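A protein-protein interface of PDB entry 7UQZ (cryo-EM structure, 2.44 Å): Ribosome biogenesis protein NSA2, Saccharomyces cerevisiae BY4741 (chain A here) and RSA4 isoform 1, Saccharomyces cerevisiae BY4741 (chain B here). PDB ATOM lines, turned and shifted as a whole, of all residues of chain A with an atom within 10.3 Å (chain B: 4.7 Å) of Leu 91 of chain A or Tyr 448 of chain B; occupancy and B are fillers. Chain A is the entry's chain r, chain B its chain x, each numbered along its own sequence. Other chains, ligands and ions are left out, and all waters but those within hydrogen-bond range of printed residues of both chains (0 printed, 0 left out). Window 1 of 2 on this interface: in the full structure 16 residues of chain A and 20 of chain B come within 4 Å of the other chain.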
ATOM      1  N   ASP A  85     -13.137 -13.428  -8.807  1.00  0.00           N
ATOM      2  CA  ASP A  85     -13.670 -12.073  -8.761  1.00  0.00           C
ATOM      3  C   ASP A  85     -13.555 -11.414 -10.132  1.00  0.00           C
ATOM      4  O   ASP A  85     -14.116 -10.339 -10.359  1.00  0.00           O
ATOM      5  CB  ASP A  85     -12.936 -11.242  -7.704  1.00  0.00           C
ATOM      6  CG  ASP A  85     -13.679  -9.970  -7.338  1.00  0.00           C
ATOM      7  OD1 ASP A  85     -14.760 -10.067  -6.720  1.00  0.00           O
ATOM      8  OD2 ASP A  85     -13.182  -8.873  -7.666  1.00  0.00           O
ATOM      9  N   ALA A  86     -12.831 -12.080 -11.035  1.00  0.00           N
ATOM     10  CA  ALA A  86     -12.555 -11.588 -12.385  1.00  0.00           C
ATOM     11  C   ALA A  86     -11.870 -10.219 -12.338  1.00  0.00           C
ATOM     12  O   ALA A  86     -12.432  -9.193 -12.722  1.00  0.00           O
ATOM     13  CB  ALA A  86     -13.830 -11.550 -13.236  1.00  0.00           C
ATOM     14  N   LEU A  87     -10.632 -10.226 -11.816  1.00  0.00           N
ATOM     15  CA  LEU A  87      -9.709  -9.113 -11.655  1.00  0.00           C
ATOM     16  C   LEU A  87      -8.789  -8.990 -12.867  1.00  0.00           C
ATOM     17  O   LEU A  87      -8.515  -9.983 -13.549  1.00  0.00           O
ATOM     18  CB  LEU A  87      -8.870  -9.303 -10.394  1.00  0.00           C
ATOM     19  CG  LEU A  87      -9.627  -9.238  -9.067  1.00  0.00           C
ATOM     20  CD1 LEU A  87      -8.709  -9.590  -7.911  1.00  0.00           C
ATOM     21  CD2 LEU A  87     -10.232  -7.858  -8.873  1.00  0.00           C
ATOM     22  N   PRO A  88      -8.292  -7.780 -13.166  1.00  0.00           N
ATOM     23  CA  PRO A  88      -7.344  -7.627 -14.281  1.00  0.00           C
ATOM     24  C   PRO A  88      -5.977  -8.212 -13.971  1.00  0.00           C
ATOM     25  O   PRO A  88      -5.753  -8.742 -12.879  1.00  0.00           O
ATOM     26  CB  PRO A  88      -7.258  -6.106 -14.471  1.00  0.00           C
ATOM     27  CG  PRO A  88      -8.387  -5.540 -13.696  1.00  0.00           C
ATOM     28  CD  PRO A  88      -8.661  -6.482 -12.584  1.00  0.00           C
ATOM     29  N   THR A  89      -5.055  -8.112 -14.932  1.00  0.00           N
ATOM     30  CA  THR A  89      -3.712  -8.650 -14.739  1.00  0.00           C
ATOM     31  C   THR A  89      -2.966  -7.913 -13.635  1.00  0.00           C
ATOM     32  O   THR A  89      -2.248  -8.530 -12.841  1.00  0.00           O
ATOM     33  CB  THR A  89      -2.925  -8.579 -16.047  1.00  0.00           C
ATOM     34  OG1 THR A  89      -3.020  -7.257 -16.591  1.00  0.00           O
ATOM     35  CG2 THR A  89      -3.461  -9.582 -17.052  1.00  0.00           C
ATOM     36  N   TYR A  90      -3.119  -6.591 -13.568  1.00  0.00           N
ATOM     37  CA  TYR A  90      -2.392  -5.805 -12.583  1.00  0.00           C
ATOM     38  C   TYR A  90      -3.004  -5.870 -11.190  1.00  0.00           C
ATOM     39  O   TYR A  90      -2.378  -5.395 -10.237  1.00  0.00           O
ATOM     40  CB  TYR A  90      -2.292  -4.344 -13.039  1.00  0.00           C
ATOM     41  CG  TYR A  90      -3.607  -3.723 -13.457  1.00  0.00           C
ATOM     42  CD1 TYR A  90      -4.431  -3.106 -12.527  1.00  0.00           C
ATOM     43  CD2 TYR A  90      -4.014  -3.741 -14.785  1.00  0.00           C
ATOM     44  CE1 TYR A  90      -5.630  -2.534 -12.903  1.00  0.00           C
ATOM     45  CE2 TYR A  90      -5.210  -3.174 -15.171  1.00  0.00           C
ATOM     46  CZ  TYR A  90      -6.014  -2.571 -14.226  1.00  0.00           C
ATOM     47  OH  TYR A  90      -7.206  -2.002 -14.605  1.00  0.00           O
ATOM     48  N   LEU A  91      -4.200  -6.442 -11.041  1.00  0.00           N
ATOM     49  CA  LEU A  91      -4.830  -6.544  -9.732  1.00  0.00           C
ATOM     50  C   LEU A  91      -4.758  -7.938  -9.125  1.00  0.00           C
ATOM     51  O   LEU A  91      -4.875  -8.063  -7.902  1.00  0.00           O
ATOM     52  CB  LEU A  91      -6.296  -6.104  -9.801  1.00  0.00           C
ATOM     53  CG  LEU A  91      -6.549  -4.606  -9.994  1.00  0.00           C
ATOM     54  CD1 LEU A  91      -7.992  -4.269  -9.668  1.00  0.00           C
ATOM     55  CD2 LEU A  91      -5.600  -3.775  -9.147  1.00  0.00           C
ATOM     56  N   LEU A  92      -4.579  -8.982  -9.930  1.00  0.00           N
ATOM     57  CA  LEU A  92      -4.318 -10.289  -9.350  1.00  0.00           C
ATOM     58  C   LEU A  92      -2.905 -10.325  -8.771  1.00  0.00           C
ATOM     59  O   LEU A  92      -2.051  -9.496  -9.102  1.00  0.00           O
ATOM     60  CB  LEU A  92      -4.523 -11.401 -10.382  1.00  0.00           C
ATOM     61  CG  LEU A  92      -3.986 -11.271 -11.807  1.00  0.00           C
ATOM     62  CD1 LEU A  92      -2.523 -11.670 -11.901  1.00  0.00           C
ATOM     63  CD2 LEU A  92      -4.834 -12.105 -12.752  1.00  0.00           C
ATOM     64  N   ASP A  93      -2.680 -11.293  -7.877  1.00  0.00           N
ATOM     65  CA  ASP A  93      -1.520 -11.361  -6.983  1.00  0.00           C
ATOM     66  C   ASP A  93      -1.467 -10.179  -6.021  1.00  0.00           C
ATOM     67  O   ASP A  93      -0.427  -9.912  -5.412  1.00  0.00           O
ATOM     68  CB  ASP A  93      -0.195 -11.482  -7.751  1.00  0.00           C
ATOM     69  CG  ASP A  93      -0.005 -12.849  -8.367  1.00  0.00           C
ATOM     70  OD1 ASP A  93      -0.637 -13.811  -7.883  1.00  0.00           O
ATOM     71  OD2 ASP A  93       0.781 -12.963  -9.331  1.00  0.00           O
ATOM     72  N   ARG A  94      -2.581  -9.466  -5.872  1.00  0.00           N
ATOM     73  CA  ARG A  94      -2.745  -8.430  -4.866  1.00  0.00           C
ATOM     74  C   ARG A  94      -4.011  -8.732  -4.082  1.00  0.00           C
ATOM     75  O   ARG A  94      -5.003  -9.198  -4.650  1.00  0.00           O
ATOM     76  CB  ARG A  94      -2.836  -7.031  -5.489  1.00  0.00           C
ATOM     77  CG  ARG A  94      -1.684  -6.667  -6.409  1.00  0.00           C
ATOM     78  CD  ARG A  94      -1.772  -5.211  -6.838  1.00  0.00           C
ATOM     79  NE  ARG A  94      -0.744  -4.859  -7.809  1.00  0.00           N
ATOM     80  CZ  ARG A  94       0.495  -4.502  -7.497  1.00  0.00           C
ATOM     81  NH1 ARG A  94       0.903  -4.447  -6.240  1.00  0.00           N
ATOM     82  NH2 ARG A  94       1.347  -4.201  -8.471  1.00  0.00           N
ATOM     83  N   GLU A  95      -3.975  -8.472  -2.783  1.00  0.00           N
ATOM     84  CA  GLU A  95      -5.112  -8.729  -1.916  1.00  0.00           C
ATOM     85  C   GLU A  95      -5.747  -7.406  -1.492  1.00  0.00           C
ATOM     86  O   GLU A  95      -5.393  -6.332  -1.991  1.00  0.00           O
ATOM     87  CB  GLU A  95      -4.680  -9.572  -0.715  1.00  0.00           C
ATOM     88  CG  GLU A  95      -4.154 -10.950  -1.086  1.00  0.00           C
ATOM     89  CD  GLU A  95      -3.870 -11.812   0.128  1.00  0.00           C
ATOM     90  OE1 GLU A  95      -4.282 -11.429   1.243  1.00  0.00           O
ATOM     91  OE2 GLU A  95      -3.232 -12.874  -0.034  1.00  0.00           O
ATOM     92  N   GLN A  96      -6.702  -7.493  -0.572  1.00  0.00           N
ATOM     93  CA  GLN A  96      -7.403  -6.316  -0.072  1.00  0.00           C
ATOM     94  C   GLN A  96      -6.475  -5.428   0.749  1.00  0.00           C
ATOM     95  O   GLN A  96      -5.454  -5.886   1.260  1.00  0.00           O
ATOM     96  CB  GLN A  96      -8.610  -6.735   0.770  1.00  0.00           C
ATOM     97  CG  GLN A  96      -9.549  -7.699   0.064  1.00  0.00           C
ATOM     98  CD  GLN A  96     -10.712  -8.125   0.938  1.00  0.00           C
ATOM     99  OE1 GLN A  96     -10.886  -7.624   2.048  1.00  0.00           O
ATOM    100  NE2 GLN A  96     -11.516  -9.057   0.438  1.00  0.00           N
ATOM    101  N   LEU A 189     -17.149  -3.725   0.420  1.00  0.00           N
ATOM    102  CA  LEU A 189     -15.688  -3.828   0.400  1.00  0.00           C
ATOM    103  C   LEU A 189     -15.108  -4.161   1.772  1.00  0.00           C
ATOM    104  O   LEU A 189     -13.909  -4.434   1.883  1.00  0.00           O
ATOM    105  CB  LEU A 189     -15.040  -2.548  -0.148  1.00  0.00           C
ATOM    106  CG  LEU A 189     -15.438  -2.099  -1.556  1.00  0.00           C
ATOM    107  CD1 LEU A 189     -14.766  -0.777  -1.900  1.00  0.00           C
ATOM    108  CD2 LEU A 189     -15.089  -3.166  -2.580  1.00  0.00           C
ATOM    109  N   ASN B 406       1.191   2.091 -11.116  1.00  0.00           N
ATOM    110  CA  ASN B 406       0.548   0.969 -11.791  1.00  0.00           C
ATOM    111  C   ASN B 406       0.783   0.995 -13.294  1.00  0.00           C
ATOM    112  O   ASN B 406       0.959  -0.061 -13.909  1.00  0.00           O
ATOM    113  CB  ASN B 406      -0.950   0.957 -11.491  1.00  0.00           C
ATOM    114  CG  ASN B 406      -1.633  -0.306 -11.981  1.00  0.00           C
ATOM    115  OD1 ASN B 406      -1.671  -1.316 -11.279  1.00  0.00           O
ATOM    116  ND2 ASN B 406      -2.180  -0.254 -13.189  1.00  0.00           N
ATOM    117  N   HIS B 407       0.783   2.176 -13.912  1.00  0.00           N
ATOM    118  CA  HIS B 407       0.882   2.237 -15.363  1.00  0.00           C
ATOM    119  C   HIS B 407       1.842   3.339 -15.779  1.00  0.00           C
ATOM    120  O   HIS B 407       2.003   4.341 -15.079  1.00  0.00           O
ATOM    121  CB  HIS B 407      -0.495   2.462 -16.004  1.00  0.00           C
ATOM    122  CG  HIS B 407      -0.556   2.094 -17.453  1.00  0.00           C
ATOM    123  ND1 HIS B 407      -0.483   3.031 -18.463  1.00  0.00           N
ATOM    124  CD2 HIS B 407      -0.682   0.894 -18.063  1.00  0.00           C
ATOM    125  CE1 HIS B 407      -0.562   2.421 -19.632  1.00  0.00           C
ATOM    126  NE2 HIS B 407      -0.684   1.124 -19.417  1.00  0.00           N
ATOM    127  N   PHE B 422      -1.091   4.590  -7.746  1.00  0.00           N
ATOM    128  CA  PHE B 422      -2.138   4.253  -6.792  1.00  0.00           C
ATOM    129  C   PHE B 422      -2.366   5.342  -5.754  1.00  0.00           C
ATOM    130  O   PHE B 422      -3.253   5.190  -4.907  1.00  0.00           O
ATOM    131  CB  PHE B 422      -1.813   2.935  -6.080  1.00  0.00           C
ATOM    132  CG  PHE B 422      -2.345   1.716  -6.777  1.00  0.00           C
ATOM    133  CD1 PHE B 422      -2.695   1.758  -8.116  1.00  0.00           C
ATOM    134  CD2 PHE B 422      -2.513   0.529  -6.086  1.00  0.00           C
ATOM    135  CE1 PHE B 422      -3.187   0.637  -8.752  1.00  0.00           C
ATOM    136  CE2 PHE B 422      -3.003  -0.595  -6.717  1.00  0.00           C
ATOM    137  CZ  PHE B 422      -3.342  -0.539  -8.052  1.00  0.00           C
ATOM    138  N   SER B 446      -7.494   5.334  -6.753  1.00  0.00           N
ATOM    139  CA  SER B 446      -6.272   4.949  -7.446  1.00  0.00           C
ATOM    140  C   SER B 446      -6.494   4.883  -8.953  1.00  0.00           C
ATOM    141  O   SER B 446      -7.501   4.352  -9.429  1.00  0.00           O
ATOM    142  CB  SER B 446      -5.774   3.599  -6.931  1.00  0.00           C
ATOM    143  OG  SER B 446      -6.677   2.561  -7.259  1.00  0.00           O
ATOM    144  N   VAL B 447      -5.545   5.434  -9.701  1.00  0.00           N
ATOM    145  CA  VAL B 447      -5.614   5.426 -11.158  1.00  0.00           C
ATOM    146  C   VAL B 447      -5.101   4.087 -11.666  1.00  0.00           C
ATOM    147  O   VAL B 447      -4.002   3.651 -11.306  1.00  0.00           O
ATOM    148  CB  VAL B 447      -4.806   6.591 -11.748  1.00  0.00           C
ATOM    149  CG1 VAL B 447      -5.161   6.792 -13.212  1.00  0.00           C
ATOM    150  CG2 VAL B 447      -5.046   7.863 -10.951  1.00  0.00           C
ATOM    151  N   TYR B 448      -5.898   3.426 -12.503  1.00  0.00           N
ATOM    152  CA  TYR B 448      -5.536   2.100 -12.988  1.00  0.00           C
ATOM    153  C   TYR B 448      -4.682   2.158 -14.250  1.00  0.00           C
ATOM    154  O   TYR B 448      -3.588   1.585 -14.279  1.00  0.00           O
ATOM    155  CB  TYR B 448      -6.798   1.267 -13.220  1.00  0.00           C
ATOM    156  CG  TYR B 448      -7.397   0.733 -11.939  1.00  0.00           C
ATOM    157  CD1 TYR B 448      -6.586   0.397 -10.862  1.00  0.00           C
ATOM    158  CD2 TYR B 448      -8.767   0.570 -11.803  1.00  0.00           C
ATOM    159  CE1 TYR B 448      -7.123  -0.089  -9.690  1.00  0.00           C
ATOM    160  CE2 TYR B 448      -9.314   0.086 -10.631  1.00  0.00           C
ATOM    161  CZ  TYR B 448      -8.487  -0.243  -9.580  1.00  0.00           C
ATOM    162  OH  TYR B 448      -9.026  -0.728  -8.411  1.00  0.00           O
ATOM    163  N   GLN B 449      -5.145   2.839 -15.296  1.00  0.00           N
ATOM    164  CA  GLN B 449      -4.326   2.957 -16.494  1.00  0.00           C
ATOM    165  C   GLN B 449      -4.686   4.225 -17.259  1.00  0.00           C
ATOM    166  O   GLN B 449      -5.660   4.925 -16.950  1.00  0.00           O
ATOM    167  CB  GLN B 449      -4.444   1.714 -17.387  1.00  0.00           C
ATOM    168  CG  GLN B 449      -5.679   1.637 -18.251  1.00  0.00           C
ATOM    169  CD  GLN B 449      -5.643   0.435 -19.173  1.00  0.00           C
ATOM    170  OE1 GLN B 449      -6.128   0.487 -20.302  1.00  0.00           O
ATOM    171  NE2 GLN B 449      -5.063  -0.659 -18.695  1.00  0.00           N
ATOM    172  N   CYS B 462      -8.372   6.189 -16.669  1.00  0.00           N
ATOM    173  CA  CYS B 462      -9.495   5.543 -16.002  1.00  0.00           C
ATOM    174  C   CYS B 462      -9.125   5.272 -14.552  1.00  0.00           C
ATOM    175  O   CYS B 462      -7.968   4.963 -14.251  1.00  0.00           O
ATOM    176  CB  CYS B 462      -9.889   4.235 -16.699  1.00  0.00           C
ATOM    177  SG  CYS B 462      -8.709   2.873 -16.530  1.00  0.00           S
ATOM    178  N   SER B 463     -10.092   5.397 -13.642  1.00  0.00           N
ATOM    179  CA  SER B 463      -9.753   5.253 -12.232  1.00  0.00           C
ATOM    180  C   SER B 463     -10.734   4.342 -11.506  1.00  0.00           C
ATOM    181  O   SER B 463     -11.793   3.971 -12.019  1.00  0.00           O
ATOM    182  CB  SER B 463      -9.691   6.616 -11.534  1.00  0.00           C
ATOM    183  OG  SER B 463      -9.474   6.473 -10.142  1.00  0.00           O
ATOM    184  N   LYS B 464     -10.337   3.984 -10.282  1.00  0.00           N
ATOM    185  CA  LYS B 464     -11.168   3.216  -9.364  1.00  0.00           C
ATOM    186  C   LYS B 464     -12.387   4.002  -8.893  1.00  0.00           C
ATOM    187  O   LYS B 464     -13.333   3.405  -8.370  1.00  0.00           O
ATOM    188  CB  LYS B 464     -10.311   2.782  -8.169  1.00  0.00           C
ATOM    189  CG  LYS B 464     -10.918   1.755  -7.233  1.00  0.00           C
ATOM    190  CD  LYS B 464     -10.052   1.585  -5.995  1.00  0.00           C
ATOM    191  CE  LYS B 464     -10.518   0.418  -5.139  1.00  0.00           C
ATOM    192  NZ  LYS B 464     -11.921   0.580  -4.677  1.00  0.00           N
ATOM    193  N   GLU B 488     -15.928   0.237 -10.788  1.00  0.00           N
ATOM    194  CA  GLU B 488     -14.545   0.537 -11.144  1.00  0.00           C
ATOM    195  C   GLU B 488     -14.292   0.276 -12.624  1.00  0.00           C
ATOM    196  O   GLU B 488     -14.790  -0.696 -13.195  1.00  0.00           O
ATOM    197  CB  GLU B 488     -13.588  -0.302 -10.298  1.00  0.00           C
ATOM    198  CG  GLU B 488     -13.869  -0.266  -8.806  1.00  0.00           C
ATOM    199  CD  GLU B 488     -12.870  -1.079  -8.007  1.00  0.00           C
ATOM    200  OE1 GLU B 488     -11.843  -1.493  -8.583  1.00  0.00           O
ATOM    201  OE2 GLU B 488     -13.110  -1.303  -6.803  1.00  0.00           O
ATOM    202  N   VAL B 489     -13.512   1.158 -13.242  1.00  0.00           N
ATOM    203  CA  VAL B 489     -13.158   1.052 -14.652  1.00  0.00           C
ATOM    204  C   VAL B 489     -11.766   0.445 -14.741  1.00  0.00           C
ATOM    205  O   VAL B 489     -10.806   0.986 -14.179  1.00  0.00           O
ATOM    206  CB  VAL B 489     -13.209   2.421 -15.349  1.00  0.00           C
ATOM    207  CG1 VAL B 489     -13.043   2.257 -16.849  1.00  0.00           C
ATOM    208  CG2 VAL B 489     -14.507   3.134 -15.019  1.00  0.00           C
ATOM    209  N   TYR B 490     -11.652  -0.676 -15.449  1.00  0.00           N
ATOM    210  CA  TYR B 490     -10.402  -1.417 -15.518  1.00  0.00           C
ATOM    211  C   TYR B 490      -9.593  -1.144 -16.775  1.00  0.00           C
ATOM    212  O   TYR B 490      -8.360  -1.109 -16.704  1.00  0.00           O
ATOM    213  CB  TYR B 490     -10.675  -2.922 -15.419  1.00  0.00           C
ATOM    214  CG  TYR B 490     -11.018  -3.382 -14.026  1.00  0.00           C
ATOM    215  CD1 TYR B 490     -10.543  -2.701 -12.913  1.00  0.00           C
ATOM    216  CD2 TYR B 490     -11.813  -4.501 -13.819  1.00  0.00           C
ATOM    217  CE1 TYR B 490     -10.849  -3.116 -11.637  1.00  0.00           C
ATOM    218  CE2 TYR B 490     -12.123  -4.925 -12.545  1.00  0.00           C
ATOM    219  CZ  TYR B 490     -11.642  -4.229 -11.458  1.00  0.00           C
ATOM    220  OH  TYR B 490     -11.952  -4.648 -10.186  1.00  0.00           O
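OH of Tyr 90 of chain A lies within hydrogen-bond range of O of Tyr 490 of chain B (2.6 Å).
The backbone carbonyl oxygen (O) of Tyr 448 of chain B lies within hydrogen-bond range of the side-chain amide nitrogen (ND2) of Asn 406 of chain B (2.6 Å). N of Tyr 448 of chain B sits at hydrogen-bond distance from O of Cys 462 of chain B, 3.1 Å away. The side-chain carboxylate (OE1) of Glu 488 of chain B is in hydrogen-bond range of the side-chain hydroxyl (OH) of Tyr 448 of chain B, 2.9 Å away. NE of Arg 94 of chain A is in hydrogen-bond range of O of Tyr 90 of chain A, 3.0 Å away.
OH of Tyr 490 of chain B touches CD2 of Leu 87 of chain A, at 3.9 Å. CG of Tyr 490 of chain B touches CG of Pro 88 of chain A, at 3.4 Å. Tyr 90 of chain A touches Asn 406 of chain B. Tyr 90 of chain A touches Tyr 448 of chain B. Leu 91 of chain A touches Tyr 448 of chain B (CD1 to OH, 3.9 Å). CD1 of Leu 91 of chain A touches CE1 of Tyr 490 of chain B, at 3.7 Å.
Leu 91 of chain A touches just these residues of chain B: Tyr 448 and Tyr 490. Of chain A, only Tyr 90 and Leu 91 come within 4 Å of Tyr 448 of chain B. Of chain A, only Tyr 90 comes within 4 Å of Asn 406 of chain B. No residue of chain A comes within 4 Å of Ser 446 of chain B. No residue of chain A comes within 4 Å of Cys 462 of chain B. No residue of chain A comes within 4 Å of Ser 463 of chain B. No residue of chain A comes within 4 Å of Lys 464 of chain B. Tyr 490 of chain B touches four residues of chain A. Of the printed residues of chain B, Tyr 90 of chain A touches Asn 406 (3.5 Å), Tyr 448 (3.6 Å) and Tyr 490 (2.6 Å). Printed residues of chain B within 4 Å of Pro 88 of chain A: Tyr 490. Of the printed residues of chain B, Leu 87 of chain A touches Tyr 490. Asp 85 of chain A touches none of the printed residues of chain B. The nearest residue of chain B that does not touch Leu 91 of chain A is Phe 422 of chain B (4.1 Å). The nearest printed residue of chain B that does not touch Tyr 90 of chain A is Gln 449 of chain B (4.3 Å).
Hydrophobic or aromatic side chains of chain B within 4 Å of the printed part of chain A: Tyr 448 and Tyr 490. Of the 13 printed residues of chain A, 4 touch a printed residue of chain B. Printed residues of chain A that touch a printed residue of chain B: Leu 87, Pro 88, Tyr 90 and Leu 91. Hydrophobic or aromatic side chains of chain A within 4 Å of the printed part of chain B: Leu 87, Pro 88, Tyr 90 and Leu 91.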
